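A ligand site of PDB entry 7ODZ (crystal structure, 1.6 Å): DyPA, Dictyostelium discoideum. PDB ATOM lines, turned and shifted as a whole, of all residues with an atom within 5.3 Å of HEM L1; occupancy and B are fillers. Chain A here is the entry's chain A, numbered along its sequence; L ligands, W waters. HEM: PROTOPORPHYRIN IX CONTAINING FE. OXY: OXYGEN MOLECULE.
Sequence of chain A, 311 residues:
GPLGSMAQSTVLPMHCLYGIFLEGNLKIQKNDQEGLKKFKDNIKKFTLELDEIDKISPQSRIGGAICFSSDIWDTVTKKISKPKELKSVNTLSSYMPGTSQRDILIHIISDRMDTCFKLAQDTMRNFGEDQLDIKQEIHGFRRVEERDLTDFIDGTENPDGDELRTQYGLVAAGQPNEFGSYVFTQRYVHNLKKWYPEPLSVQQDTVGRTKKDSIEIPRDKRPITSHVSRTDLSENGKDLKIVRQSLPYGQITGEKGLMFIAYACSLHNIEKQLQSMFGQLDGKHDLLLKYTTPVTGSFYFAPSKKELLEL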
ATOM      1  N   ASP A 148      35.901  -1.777  -1.292  1.00  0.00           N
ATOM      2  CA  ASP A 148      35.194  -2.275  -0.113  1.00  0.00           C
ATOM      3  C   ASP A 148      35.292  -3.795  -0.108  1.00  0.00           C
ATOM      4  O   ASP A 148      35.625  -4.418  -1.114  1.00  0.00           O
ATOM      5  CB  ASP A 148      33.730  -1.801  -0.180  1.00  0.00           C
ATOM      6  CG  ASP A 148      32.861  -2.437   0.889  1.00  0.00           C
ATOM      7  OD1 ASP A 148      32.895  -1.966   2.048  1.00  0.00           O
ATOM      8  OD2 ASP A 148      32.131  -3.393   0.552  1.00  0.00           O
ATOM      9  N   THR A 150      33.015  -5.900  -0.275  1.00  0.00           N
ATOM     10  CA  THR A 150      32.227  -6.448  -1.383  1.00  0.00           C
ATOM     11  C   THR A 150      33.033  -6.604  -2.662  1.00  0.00           C
ATOM     12  O   THR A 150      32.541  -7.220  -3.620  1.00  0.00           O
ATOM     13  CB  THR A 150      31.041  -5.551  -1.717  1.00  0.00           C
ATOM     14  OG1 THR A 150      31.534  -4.230  -2.026  1.00  0.00           O
ATOM     15  CG2 THR A 150      30.017  -5.498  -0.577  1.00  0.00           C
ATOM     16  N   PHE A 152      33.751  -4.138  -4.638  1.00  0.00           N
ATOM     17  CA  PHE A 152      33.470  -2.982  -5.462  1.00  0.00           C
ATOM     18  C   PHE A 152      34.314  -1.798  -5.026  1.00  0.00           C
ATOM     19  O   PHE A 152      34.543  -1.596  -3.827  1.00  0.00           O
ATOM     20  CB  PHE A 152      31.987  -2.602  -5.383  1.00  0.00           C
ATOM     21  CG  PHE A 152      31.109  -3.448  -6.253  1.00  0.00           C
ATOM     22  CD1 PHE A 152      30.927  -4.792  -5.972  1.00  0.00           C
ATOM     23  CD2 PHE A 152      30.478  -2.910  -7.376  1.00  0.00           C
ATOM     24  CE1 PHE A 152      30.140  -5.599  -6.787  1.00  0.00           C
ATOM     25  CE2 PHE A 152      29.682  -3.707  -8.197  1.00  0.00           C
ATOM     26  CZ  PHE A 152      29.509  -5.047  -7.906  1.00  0.00           C
ATOM     27  N   ILE A 153      34.764  -0.990  -5.994  1.00  0.00           N
ATOM     28  CA  ILE A 153      35.464   0.239  -5.655  1.00  0.00           C
ATOM     29  C   ILE A 153      34.520   1.167  -4.904  1.00  0.00           C
ATOM     30  O   ILE A 153      33.392   1.397  -5.328  1.00  0.00           O
ATOM     31  CB  ILE A 153      35.988   0.907  -6.935  1.00  0.00           C
ATOM     32  CG1 ILE A 153      37.030   0.037  -7.616  1.00  0.00           C
ATOM     33  CG2 ILE A 153      36.554   2.306  -6.642  1.00  0.00           C
ATOM     34  CD1 ILE A 153      37.231   0.392  -9.073  1.00  0.00           C
ATOM     35  N   ASP A 154      34.988   1.716  -3.769  1.00  0.00           N
ATOM     36  CA  ASP A 154      34.203   2.639  -2.951  1.00  0.00           C
ATOM     37  C   ASP A 154      34.819   4.023  -3.108  1.00  0.00           C
ATOM     38  O   ASP A 154      35.970   4.227  -2.687  1.00  0.00           O
ATOM     39  CB  ASP A 154      34.184   2.204  -1.483  1.00  0.00           C
ATOM     40  CG  ASP A 154      33.277   3.087  -0.612  1.00  0.00           C
ATOM     41  OD1 ASP A 154      32.343   3.718  -1.135  1.00  0.00           O
ATOM     42  OD2 ASP A 154      33.498   3.128   0.623  1.00  0.00           O
ATOM     43  N   GLY A 155      34.086   4.953  -3.711  1.00  0.00           N
ATOM     44  CA  GLY A 155      34.539   6.333  -3.819  1.00  0.00           C
ATOM     45  C   GLY A 155      34.416   6.980  -5.184  1.00  0.00           C
ATOM     46  O   GLY A 155      34.673   8.181  -5.330  1.00  0.00           O
ATOM     47  N   THR A 156      33.996   6.216  -6.199  1.00  0.00           N
ATOM     48  CA  THR A 156      33.967   6.702  -7.576  1.00  0.00           C
ATOM     49  C   THR A 156      33.281   8.068  -7.698  1.00  0.00           C
ATOM     50  O   THR A 156      33.812   8.966  -8.353  1.00  0.00           O
ATOM     51  CB  THR A 156      33.266   5.680  -8.468  1.00  0.00           C
ATOM     52  OG1 THR A 156      33.964   4.435  -8.349  1.00  0.00           O
ATOM     53  CG2 THR A 156      33.276   6.116  -9.937  1.00  0.00           C
ATOM     54  N   GLU A 157      32.116   8.226  -7.075  1.00  0.00           N
ATOM     55  CA  GLU A 157      31.359   9.471  -7.205  1.00  0.00           C
ATOM     56  C   GLU A 157      31.487  10.393  -5.999  1.00  0.00           C
ATOM     57  O   GLU A 157      30.732  11.367  -5.886  1.00  0.00           O
ATOM     58  CB  GLU A 157      29.887   9.175  -7.494  1.00  0.00           C
ATOM     59  CG  GLU A 157      29.681   8.539  -8.864  1.00  0.00           C
ATOM     60  CD  GLU A 157      30.045   9.481 -10.010  1.00  0.00           C
ATOM     61  OE1 GLU A 157      29.818  10.698  -9.883  1.00  0.00           O
ATOM     62  OE2 GLU A 157      30.565   8.987 -11.034  1.00  0.00           O
ATOM     63  N   ASN A 158      32.406  10.099  -5.092  1.00  0.00           N
ATOM     64  CA  ASN A 158      32.784  11.073  -4.068  1.00  0.00           C
ATOM     65  C   ASN A 158      33.208  12.366  -4.743  1.00  0.00           C
ATOM     66  O   ASN A 158      33.965  12.341  -5.722  1.00  0.00           O
ATOM     67  CB  ASN A 158      33.945  10.510  -3.249  1.00  0.00           C
ATOM     68  CG  ASN A 158      33.749  10.629  -1.761  1.00  0.00           C
ATOM     69  OD1 ASN A 158      32.745  11.140  -1.276  1.00  0.00           O
ATOM     70  ND2 ASN A 158      34.722  10.133  -1.025  1.00  0.00           N
ATOM     71  N   PHE A 184      28.474  11.837  10.166  1.00  0.00           N
ATOM     72  CA  PHE A 184      27.708  10.651  10.465  1.00  0.00           C
ATOM     73  C   PHE A 184      28.654   9.463  10.410  1.00  0.00           C
ATOM     74  O   PHE A 184      29.344   9.277   9.409  1.00  0.00           O
ATOM     75  CB  PHE A 184      26.574  10.445   9.454  1.00  0.00           C
ATOM     76  CG  PHE A 184      25.849   9.119   9.594  1.00  0.00           C
ATOM     77  CD1 PHE A 184      25.177   8.778  10.757  1.00  0.00           C
ATOM     78  CD2 PHE A 184      25.846   8.211   8.531  1.00  0.00           C
ATOM     79  CE1 PHE A 184      24.501   7.564  10.860  1.00  0.00           C
ATOM     80  CE2 PHE A 184      25.172   7.015   8.626  1.00  0.00           C
ATOM     81  CZ  PHE A 184      24.490   6.683   9.782  1.00  0.00           C
ATOM     82  N   GLN A 186      28.904   5.136  11.049  1.00  0.00           N
ATOM     83  CA  GLN A 186      28.052   3.954  11.112  1.00  0.00           C
ATOM     84  C   GLN A 186      28.914   2.756  10.771  1.00  0.00           C
ATOM     85  O   GLN A 186      29.414   2.664   9.650  1.00  0.00           O
ATOM     86  CB  GLN A 186      26.905   4.083  10.120  1.00  0.00           C
ATOM     87  CG  GLN A 186      25.854   3.004  10.216  1.00  0.00           C
ATOM     88  CD  GLN A 186      24.665   3.326   9.333  1.00  0.00           C
ATOM     89  OE1 GLN A 186      24.827   3.732   8.173  1.00  0.00           O
ATOM     90  NE2 GLN A 186      23.475   3.167   9.875  1.00  0.00           N
ATOM     91  N   TYR A 188      29.419  -0.972   9.734  1.00  0.00           N
ATOM     92  CA  TYR A 188      28.718  -2.068   9.097  1.00  0.00           C
ATOM     93  C   TYR A 188      29.469  -3.375   9.305  1.00  0.00           C
ATOM     94  O   TYR A 188      30.703  -3.415   9.251  1.00  0.00           O
ATOM     95  CB  TYR A 188      28.552  -1.824   7.589  1.00  0.00           C
ATOM     96  CG  TYR A 188      27.422  -0.874   7.285  1.00  0.00           C
ATOM     97  CD1 TYR A 188      27.631   0.503   7.324  1.00  0.00           C
ATOM     98  CD2 TYR A 188      26.170  -1.345   6.959  1.00  0.00           C
ATOM     99  CE1 TYR A 188      26.585   1.386   7.060  1.00  0.00           C
ATOM    100  CE2 TYR A 188      25.124  -0.485   6.694  1.00  0.00           C
ATOM    101  CZ  TYR A 188      25.344   0.879   6.731  1.00  0.00           C
ATOM    102  OH  TYR A 188      24.287   1.717   6.465  1.00  0.00           O
ATOM    103  N   HIS A 190      29.695  -6.887   7.425  1.00  0.00           N
ATOM    104  CA  HIS A 190      29.353  -7.562   6.174  1.00  0.00           C
ATOM    105  C   HIS A 190      29.103  -9.045   6.388  1.00  0.00           C
ATOM    106  O   HIS A 190      29.764  -9.705   7.203  1.00  0.00           O
ATOM    107  CB  HIS A 190      30.494  -7.418   5.162  1.00  0.00           C
ATOM    108  CG  HIS A 190      30.636  -6.044   4.572  1.00  0.00           C
ATOM    109  ND1 HIS A 190      29.965  -4.940   5.034  1.00  0.00           N
ATOM    110  CD2 HIS A 190      31.405  -5.627   3.538  1.00  0.00           C
ATOM    111  CE1 HIS A 190      30.298  -3.893   4.297  1.00  0.00           C
ATOM    112  NE2 HIS A 190      31.173  -4.276   3.389  1.00  0.00           N
ATOM    113  N   VAL A 207      24.581  -2.936  -6.401  1.00  0.00           N
ATOM    114  CA  VAL A 207      25.337  -1.708  -6.187  1.00  0.00           C
ATOM    115  C   VAL A 207      24.867  -0.606  -7.136  1.00  0.00           C
ATOM    116  O   VAL A 207      24.685   0.546  -6.727  1.00  0.00           O
ATOM    117  CB  VAL A 207      26.837  -1.972  -6.346  1.00  0.00           C
ATOM    118  CG1 VAL A 207      27.621  -0.651  -6.323  1.00  0.00           C
ATOM    119  CG2 VAL A 207      27.320  -2.904  -5.254  1.00  0.00           C
ATOM    120  N   ARG A 209      26.641  -0.201 -10.180  1.00  0.00           N
ATOM    121  CA  ARG A 209      27.808   0.073 -11.015  1.00  0.00           C
ATOM    122  C   ARG A 209      28.447  -1.254 -11.368  1.00  0.00           C
ATOM    123  O   ARG A 209      28.174  -2.279 -10.733  1.00  0.00           O
ATOM    124  CB  ARG A 209      28.850   0.972 -10.300  1.00  0.00           C
ATOM    125  CG  ARG A 209      28.262   2.189  -9.594  1.00  0.00           C
ATOM    126  CD  ARG A 209      29.346   3.119  -9.035  1.00  0.00           C
ATOM    127  NE  ARG A 209      30.055   3.773 -10.123  1.00  0.00           N
ATOM    128  CZ  ARG A 209      29.662   4.908 -10.696  1.00  0.00           C
ATOM    129  NH1 ARG A 209      28.580   5.553 -10.273  1.00  0.00           N
ATOM    130  NH2 ARG A 209      30.357   5.397 -11.713  1.00  0.00           N
ATOM    131  N   SER A 214      33.757   0.041 -12.098  1.00  0.00           N
ATOM    132  CA  SER A 214      32.866   1.021 -11.457  1.00  0.00           C
ATOM    133  C   SER A 214      32.206   1.935 -12.483  1.00  0.00           C
ATOM    134  O   SER A 214      32.108   3.153 -12.286  1.00  0.00           O
ATOM    135  CB  SER A 214      33.611   1.824 -10.386  1.00  0.00           C
ATOM    136  OG  SER A 214      32.685   2.448  -9.521  1.00  0.00           O
ATOM    137  N   HIS A 227      22.009   0.488  -4.772  1.00  0.00           N
ATOM    138  CA  HIS A 227      22.610   1.425  -3.845  1.00  0.00           C
ATOM    139  C   HIS A 227      22.757   2.821  -4.457  1.00  0.00           C
ATOM    140  O   HIS A 227      22.417   3.823  -3.819  1.00  0.00           O
ATOM    141  CB  HIS A 227      23.952   0.895  -3.372  1.00  0.00           C
ATOM    142  CG  HIS A 227      24.579   1.725  -2.316  1.00  0.00           C
ATOM    143  ND1 HIS A 227      23.954   2.019  -1.129  1.00  0.00           N
ATOM    144  CD2 HIS A 227      25.786   2.339  -2.278  1.00  0.00           C
ATOM    145  CE1 HIS A 227      24.746   2.775  -0.391  1.00  0.00           C
ATOM    146  NE2 HIS A 227      25.860   2.979  -1.062  1.00  0.00           N
ATOM    147  N   VAL A 228      23.222   2.903  -5.710  1.00  0.00           N
ATOM    148  CA  VAL A 228      23.363   4.210  -6.345  1.00  0.00           C
ATOM    149  C   VAL A 228      21.995   4.885  -6.486  1.00  0.00           C
ATOM    150  O   VAL A 228      21.870   6.098  -6.257  1.00  0.00           O
ATOM    151  CB  VAL A 228      24.063   4.081  -7.705  1.00  0.00           C
ATOM    152  CG1 VAL A 228      24.067   5.428  -8.422  1.00  0.00           C
ATOM    153  CG2 VAL A 228      25.500   3.576  -7.501  1.00  0.00           C
ATOM    154  N   THR A 231      21.048   6.428  -3.117  1.00  0.00           N
ATOM    155  CA  THR A 231      21.871   7.488  -2.529  1.00  0.00           C
ATOM    156  C   THR A 231      22.139   8.677  -3.444  1.00  0.00           C
ATOM    157  O   THR A 231      22.532   9.734  -2.951  1.00  0.00           O
ATOM    158  CB  THR A 231      23.225   6.918  -2.067  1.00  0.00           C
ATOM    159  OG1 THR A 231      23.885   6.312  -3.177  1.00  0.00           O
ATOM    160  CG2 THR A 231      23.021   5.887  -0.958  1.00  0.00           C
ATOM    161  N   ASP A 232      21.943   8.538  -4.759  1.00  0.00           N
ATOM    162  CA  ASP A 232      22.122   9.660  -5.692  1.00  0.00           C
ATOM    163  C   ASP A 232      20.819  10.429  -5.743  1.00  0.00           C
ATOM    164  O   ASP A 232      19.961  10.222  -6.607  1.00  0.00           O
ATOM    165  CB  ASP A 232      22.548   9.151  -7.059  1.00  0.00           C
ATOM    166  CG  ASP A 232      22.764  10.264  -8.071  1.00  0.00           C
ATOM    167  OD1 ASP A 232      22.803  11.455  -7.695  1.00  0.00           O
ATOM    168  OD2 ASP A 232      22.901   9.936  -9.268  1.00  0.00           O
ATOM    169  N   LYS A 241      24.747  15.942  -2.229  1.00  0.00           N
ATOM    170  CA  LYS A 241      26.007  15.218  -2.165  1.00  0.00           C
ATOM    171  C   LYS A 241      26.627  15.317  -0.777  1.00  0.00           C
ATOM    172  O   LYS A 241      26.349  16.238   0.006  1.00  0.00           O
ATOM    173  CB  LYS A 241      26.985  15.738  -3.221  1.00  0.00           C
ATOM    174  CG  LYS A 241      26.515  15.460  -4.646  1.00  0.00           C
ATOM    175  CD  LYS A 241      27.508  15.935  -5.676  1.00  0.00           C
ATOM    176  CE  LYS A 241      27.104  15.474  -7.073  1.00  0.00           C
ATOM    177  NZ  LYS A 241      26.915  13.994  -7.112  1.00  0.00           N
ATOM    178  N   ILE A 242      27.472  14.327  -0.475  1.00  0.00           N
ATOM    179  CA  ILE A 242      28.186  14.246   0.795  1.00  0.00           C
ATOM    180  C   ILE A 242      29.622  13.837   0.492  1.00  0.00           C
ATOM    181  O   ILE A 242      29.956  13.411  -0.616  1.00  0.00           O
ATOM    182  CB  ILE A 242      27.539  13.237   1.770  1.00  0.00           C
ATOM    183  CG1 ILE A 242      27.593  11.830   1.181  1.00  0.00           C
ATOM    184  CG2 ILE A 242      26.086  13.664   2.106  1.00  0.00           C
ATOM    185  CD1 ILE A 242      26.958  10.758   2.100  1.00  0.00           C
ATOM    186  N   ARG A 244      32.464  11.311   1.654  1.00  0.00           N
ATOM    187  CA  ARG A 244      32.659  10.080   2.398  1.00  0.00           C
ATOM    188  C   ARG A 244      34.148   9.817   2.647  1.00  0.00           C
ATOM    189  O   ARG A 244      34.976  10.074   1.777  1.00  0.00           O
ATOM    190  CB  ARG A 244      32.051   8.897   1.653  1.00  0.00           C
ATOM    191  CG  ARG A 244      30.510   8.934   1.658  1.00  0.00           C
ATOM    192  CD  ARG A 244      29.952   7.925   0.662  1.00  0.00           C
ATOM    193  NE  ARG A 244      30.181   8.333  -0.726  1.00  0.00           N
ATOM    194  CZ  ARG A 244      30.588   7.518  -1.699  1.00  0.00           C
ATOM    195  NH1 ARG A 244      30.842   6.235  -1.454  1.00  0.00           N
ATOM    196  NH2 ARG A 244      30.774   7.999  -2.927  1.00  0.00           N
ATOM    197  N   LEU A 258      32.613  -2.346   6.759  1.00  0.00           N
ATOM    198  CA  LEU A 258      32.934  -0.994   6.342  1.00  0.00           C
ATOM    199  C   LEU A 258      32.680  -0.071   7.518  1.00  0.00           C
ATOM    200  O   LEU A 258      31.603  -0.105   8.110  1.00  0.00           O
ATOM    201  CB  LEU A 258      32.073  -0.545   5.150  1.00  0.00           C
ATOM    202  CG  LEU A 258      32.430   0.865   4.654  1.00  0.00           C
ATOM    203  CD1 LEU A 258      33.758   0.866   3.934  1.00  0.00           C
ATOM    204  CD2 LEU A 258      31.345   1.418   3.717  1.00  0.00           C
ATOM    205  N   PHE A 260      31.730   3.266   7.972  1.00  0.00           N
ATOM    206  CA  PHE A 260      31.198   4.351   7.179  1.00  0.00           C
ATOM    207  C   PHE A 260      31.350   5.673   7.910  1.00  0.00           C
ATOM    208  O   PHE A 260      31.038   5.773   9.110  1.00  0.00           O
ATOM    209  CB  PHE A 260      29.724   4.121   6.844  1.00  0.00           C
ATOM    210  CG  PHE A 260      29.172   5.179   5.948  1.00  0.00           C
ATOM    211  CD1 PHE A 260      29.294   5.069   4.577  1.00  0.00           C
ATOM    212  CD2 PHE A 260      28.587   6.323   6.486  1.00  0.00           C
ATOM    213  CE1 PHE A 260      28.803   6.078   3.730  1.00  0.00           C
ATOM    214  CE2 PHE A 260      28.113   7.341   5.661  1.00  0.00           C
ATOM    215  CZ  PHE A 260      28.226   7.204   4.279  1.00  0.00           C
ATOM    216  N   ILE A 270      22.715  13.904   4.476  1.00  0.00           N
ATOM    217  CA  ILE A 270      22.953  12.546   4.950  1.00  0.00           C
ATOM    218  C   ILE A 270      21.640  11.886   5.338  1.00  0.00           C
ATOM    219  O   ILE A 270      21.366  10.740   4.961  1.00  0.00           O
ATOM    220  CB  ILE A 270      23.919  12.567   6.138  1.00  0.00           C
ATOM    221  CG1 ILE A 270      25.258  13.178   5.723  1.00  0.00           C
ATOM    222  CG2 ILE A 270      24.122  11.146   6.683  1.00  0.00           C
ATOM    223  CD1 ILE A 270      26.176  13.520   6.896  1.00  0.00           C
ATOM    224  N   GLN A 273      19.436  10.440   2.628  1.00  0.00           N
ATOM    225  CA  GLN A 273      19.940   9.180   2.088  1.00  0.00           C
ATOM    226  C   GLN A 273      19.635   8.031   3.032  1.00  0.00           C
ATOM    227  O   GLN A 273      19.334   6.912   2.590  1.00  0.00           O
ATOM    228  CB  GLN A 273      21.442   9.285   1.818  1.00  0.00           C
ATOM    229  CG  GLN A 273      21.766  10.348   0.774  1.00  0.00           C
ATOM    230  CD  GLN A 273      23.228  10.387   0.451  1.00  0.00           C
ATOM    231  OE1 GLN A 273      23.926   9.374   0.519  1.00  0.00           O
ATOM    232  NE2 GLN A 273      23.724  11.564   0.079  1.00  0.00           N
ATOM    233  N   LEU A 274      19.718   8.274   4.352  1.00  0.00           N
ATOM    234  CA  LEU A 274      19.372   7.224   5.305  1.00  0.00           C
ATOM    235  C   LEU A 274      17.890   6.871   5.215  1.00  0.00           C
ATOM    236  O   LEU A 274      17.527   5.696   5.281  1.00  0.00           O
ATOM    237  CB  LEU A 274      19.741   7.654   6.722  1.00  0.00           C
ATOM    238  CG  LEU A 274      21.231   7.883   6.924  1.00  0.00           C
ATOM    239  CD1 LEU A 274      21.456   8.390   8.353  1.00  0.00           C
ATOM    240  CD2 LEU A 274      22.046   6.627   6.660  1.00  0.00           C
ATOM    241  N   MET A 277      17.659   4.683   2.069  1.00  0.00           N
ATOM    242  CA  MET A 277      18.249   3.336   2.163  1.00  0.00           C
ATOM    243  C   MET A 277      17.432   2.435   3.071  1.00  0.00           C
ATOM    244  O   MET A 277      17.315   1.226   2.826  1.00  0.00           O
ATOM    245  CB  MET A 277      19.674   3.428   2.685  1.00  0.00           C
ATOM    246  CG  MET A 277      20.661   3.952   1.685  1.00  0.00           C
ATOM    247  SD  MET A 277      22.301   4.133   2.410  1.00  0.00           S
ATOM    248  CE  MET A 277      22.690   2.426   2.843  1.00  0.00           C
ATOM    249  N   LEU A 288      21.717  -3.389  -0.920  1.00  0.00           N
ATOM    250  CA  LEU A 288      22.963  -3.694  -0.217  1.00  0.00           C
ATOM    251  C   LEU A 288      22.700  -4.214   1.188  1.00  0.00           C
ATOM    252  O   LEU A 288      23.498  -4.992   1.726  1.00  0.00           O
ATOM    253  CB  LEU A 288      23.850  -2.453  -0.201  1.00  0.00           C
ATOM    254  CG  LEU A 288      25.359  -2.556  -0.098  1.00  0.00           C
ATOM    255  CD1 LEU A 288      25.915  -3.560  -1.104  1.00  0.00           C
ATOM    256  CD2 LEU A 288      25.912  -1.168  -0.351  1.00  0.00           C
ATOM    257  N   THR A 292      24.760  -6.674   4.469  1.00  0.00           N
ATOM    258  CA  THR A 292      25.527  -5.979   5.486  1.00  0.00           C
ATOM    259  C   THR A 292      24.541  -5.336   6.443  1.00  0.00           C
ATOM    260  O   THR A 292      23.390  -5.084   6.084  1.00  0.00           O
ATOM    261  CB  THR A 292      26.481  -4.952   4.860  1.00  0.00           C
ATOM    262  OG1 THR A 292      27.319  -4.400   5.873  1.00  0.00           O
ATOM    263  CG2 THR A 292      25.703  -3.834   4.174  1.00  0.00           C
HETATM  264  CHA HEM L   1      28.309   4.977  -3.538  1.00  0.00           C
HETATM  265  CHB HEM L   1      29.464   0.995  -1.000  1.00  0.00           C
HETATM  266  CHC HEM L   1      26.890   2.730   2.803  1.00  0.00           C
HETATM  267  CHD HEM L   1      26.286   6.911   0.421  1.00  0.00           C
HETATM  268  C1A HEM L   1      28.779   3.743  -3.150  1.00  0.00           C
HETATM  269  C2A HEM L   1      29.436   2.851  -4.044  1.00  0.00           C
HETATM  270  C3A HEM L   1      29.761   1.744  -3.339  1.00  0.00           C
HETATM  271  C4A HEM L   1      29.342   1.930  -2.010  1.00  0.00           C
HETATM  272  CMA HEM L   1      30.476   0.514  -3.864  1.00  0.00           C
HETATM  273  CAA HEM L   1      29.703   3.098  -5.524  1.00  0.00           C
HETATM  274  CBA HEM L   1      31.048   3.812  -5.819  1.00  0.00           C
HETATM  275  CGA HEM L   1      31.027   5.250  -5.389  1.00  0.00           C
HETATM  276  O1A HEM L   1      30.519   6.147  -6.102  1.00  0.00           O
HETATM  277  O2A HEM L   1      31.542   5.562  -4.293  1.00  0.00           O
HETATM  278  C1B HEM L   1      28.838   1.137   0.242  1.00  0.00           C
HETATM  279  C2B HEM L   1      28.878   0.131   1.250  1.00  0.00           C
HETATM  280  C3B HEM L   1      28.175   0.590   2.324  1.00  0.00           C
HETATM  281  C4B HEM L   1      27.683   1.941   1.940  1.00  0.00           C
HETATM  282  CMB HEM L   1      29.611  -1.187   1.093  1.00  0.00           C
HETATM  283  CAB HEM L   1      27.899  -0.029   3.640  1.00  0.00           C
HETATM  284  CBB HEM L   1      27.999  -1.316   3.891  1.00  0.00           C
HETATM  285  C1C HEM L   1      26.495   4.031   2.498  1.00  0.00           C
HETATM  286  C2C HEM L   1      25.721   4.887   3.319  1.00  0.00           C
HETATM  287  C3C HEM L   1      25.536   6.087   2.628  1.00  0.00           C
HETATM  288  C4C HEM L   1      26.203   5.941   1.385  1.00  0.00           C
HETATM  289  CMC HEM L   1      25.231   4.506   4.687  1.00  0.00           C
HETATM  290  CAC HEM L   1      24.795   7.304   3.030  1.00  0.00           C
HETATM  291  CBC HEM L   1      24.665   7.730   4.292  1.00  0.00           C
HETATM  292  C1D HEM L   1      26.825   6.675  -0.847  1.00  0.00           C
HETATM  293  C2D HEM L   1      26.786   7.735  -1.860  1.00  0.00           C
HETATM  294  C3D HEM L   1      27.315   7.205  -2.978  1.00  0.00           C
HETATM  295  C4D HEM L   1      27.700   5.828  -2.624  1.00  0.00           C
HETATM  296  CMD HEM L   1      26.237   9.138  -1.699  1.00  0.00           C
HETATM  297  CAD HEM L   1      27.491   7.918  -4.306  1.00  0.00           C
HETATM  298  CBD HEM L   1      26.184   7.852  -5.114  1.00  0.00           C
HETATM  299  CGD HEM L   1      26.301   8.646  -6.404  1.00  0.00           C
HETATM  300  O1D HEM L   1      26.111   9.885  -6.408  1.00  0.00           O
HETATM  301  O2D HEM L   1      26.586   8.063  -7.475  1.00  0.00           O
HETATM  302  NA  HEM L   1      28.682   3.136  -1.907  1.00  0.00           N
HETATM  303  NB  HEM L   1      28.149   2.193   0.691  1.00  0.00           N
HETATM  304  NC  HEM L   1      26.722   4.669   1.323  1.00  0.00           N
HETATM  305  ND  HEM L   1      27.430   5.553  -1.336  1.00  0.00           N
HETATM  306 FE   HEM L   1      27.663   3.920  -0.378  1.00  0.00          FE
HETATM  307  O1  OXY L   2      29.815   4.503   0.493  1.00  0.00           O
HETATM  308  O2  OXY L   2      31.412   4.759   1.788  1.00  0.00           O
HETATM  309  O   HOH W   1      28.283  12.343  -5.461  1.00  0.00           O
HETATM  310  O   HOH W   2      25.164  11.518  -4.056  1.00  0.00           O
HETATM  311  O   HOH W   3      28.095   5.840  -7.444  1.00  0.00           O
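O2A of HEM L1 is in hydrogen-bond range of N of Gly 155 (2.7 Å).
A ring nitrogen (NE2) of His 227 binds an iron atom (FE) of HEM L1, 2.1 Å away.
The guanidinium group (NH2) of Arg 244 lies within salt-bridge range of an oxygen (O2A) of HEM L1.
An oxygen (O1A) of HEM L1 sits at hydrogen-bond distance from the backbone NH (N) of Glu 157 (2.8 Å).
An oxygen (O2A) of HEM L1 lies within hydrogen-bond range of the backbone NH (N) of Thr 156, at 3.2 Å.
An oxygen (O1) of OXY L2 lies close to the guanidinium group of Arg 244.
Water W3 bridges an oxygen (O2D) of HEM L1 (2.7 Å) and the guanidinium group (NH1) of Arg 209 (2.9 Å).
Water W2 bridges O1D of HEM L1 (3.0 Å) and O of Thr 231 (3.4 Å).
Water W1 lies within hydrogen-bond range of O of Glu 157, NZ of Lys 241 and O1D of HEM L1.
Merely in contact with HEM L1: Asp 148, Phe 152, Ile 153, Asp 154, Gln 186, Tyr 188, His 190, Val 207, Arg 209, Val 228, Thr 231, Asp 232, Leu 258, Phe 260, Gln 273, Leu 274, Met 277, Leu 288 and Thr 292.
The nearest printed residue that does not touch HEM L1 is Ile 242 (4.2 Å).
An oxygen (O1) of OXY L2 binds an iron atom (FE) of HEM L1 (2.4 Å).
OG1 of Thr 150 sits at hydrogen-bond distance from OD2 of Asp 148, 2.8 Å away.
The guanidinium group (NH2) of Arg 209 is in hydrogen-bond range of the backbone carbonyl oxygen (O) of Ser 214, at 2.9 Å.
The backbone NH (N) of Val 228 sits at hydrogen-bond distance from the backbone carbonyl oxygen (O) of Val 207, 3.0 Å away.
OG1 of Thr 292 lies within hydrogen-bond range of ND1 of His 190 (2.8 Å).
The backbone NH (N) of Phe 260 is in hydrogen-bond range of the backbone carbonyl oxygen (O) of Gln 186, at 2.9 Å.
The backbone carbonyl oxygen of His 227 is in hydrogen-bond range of the side-chain hydroxyl of Thr 231 (3.0 Å).
The backbone NH (N) of Tyr 188 is in hydrogen-bond range of the backbone carbonyl oxygen (O) of Leu 258, 2.9 Å away.
N of His 227 lies within hydrogen-bond range of O of Val 207, 3.3 Å away.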
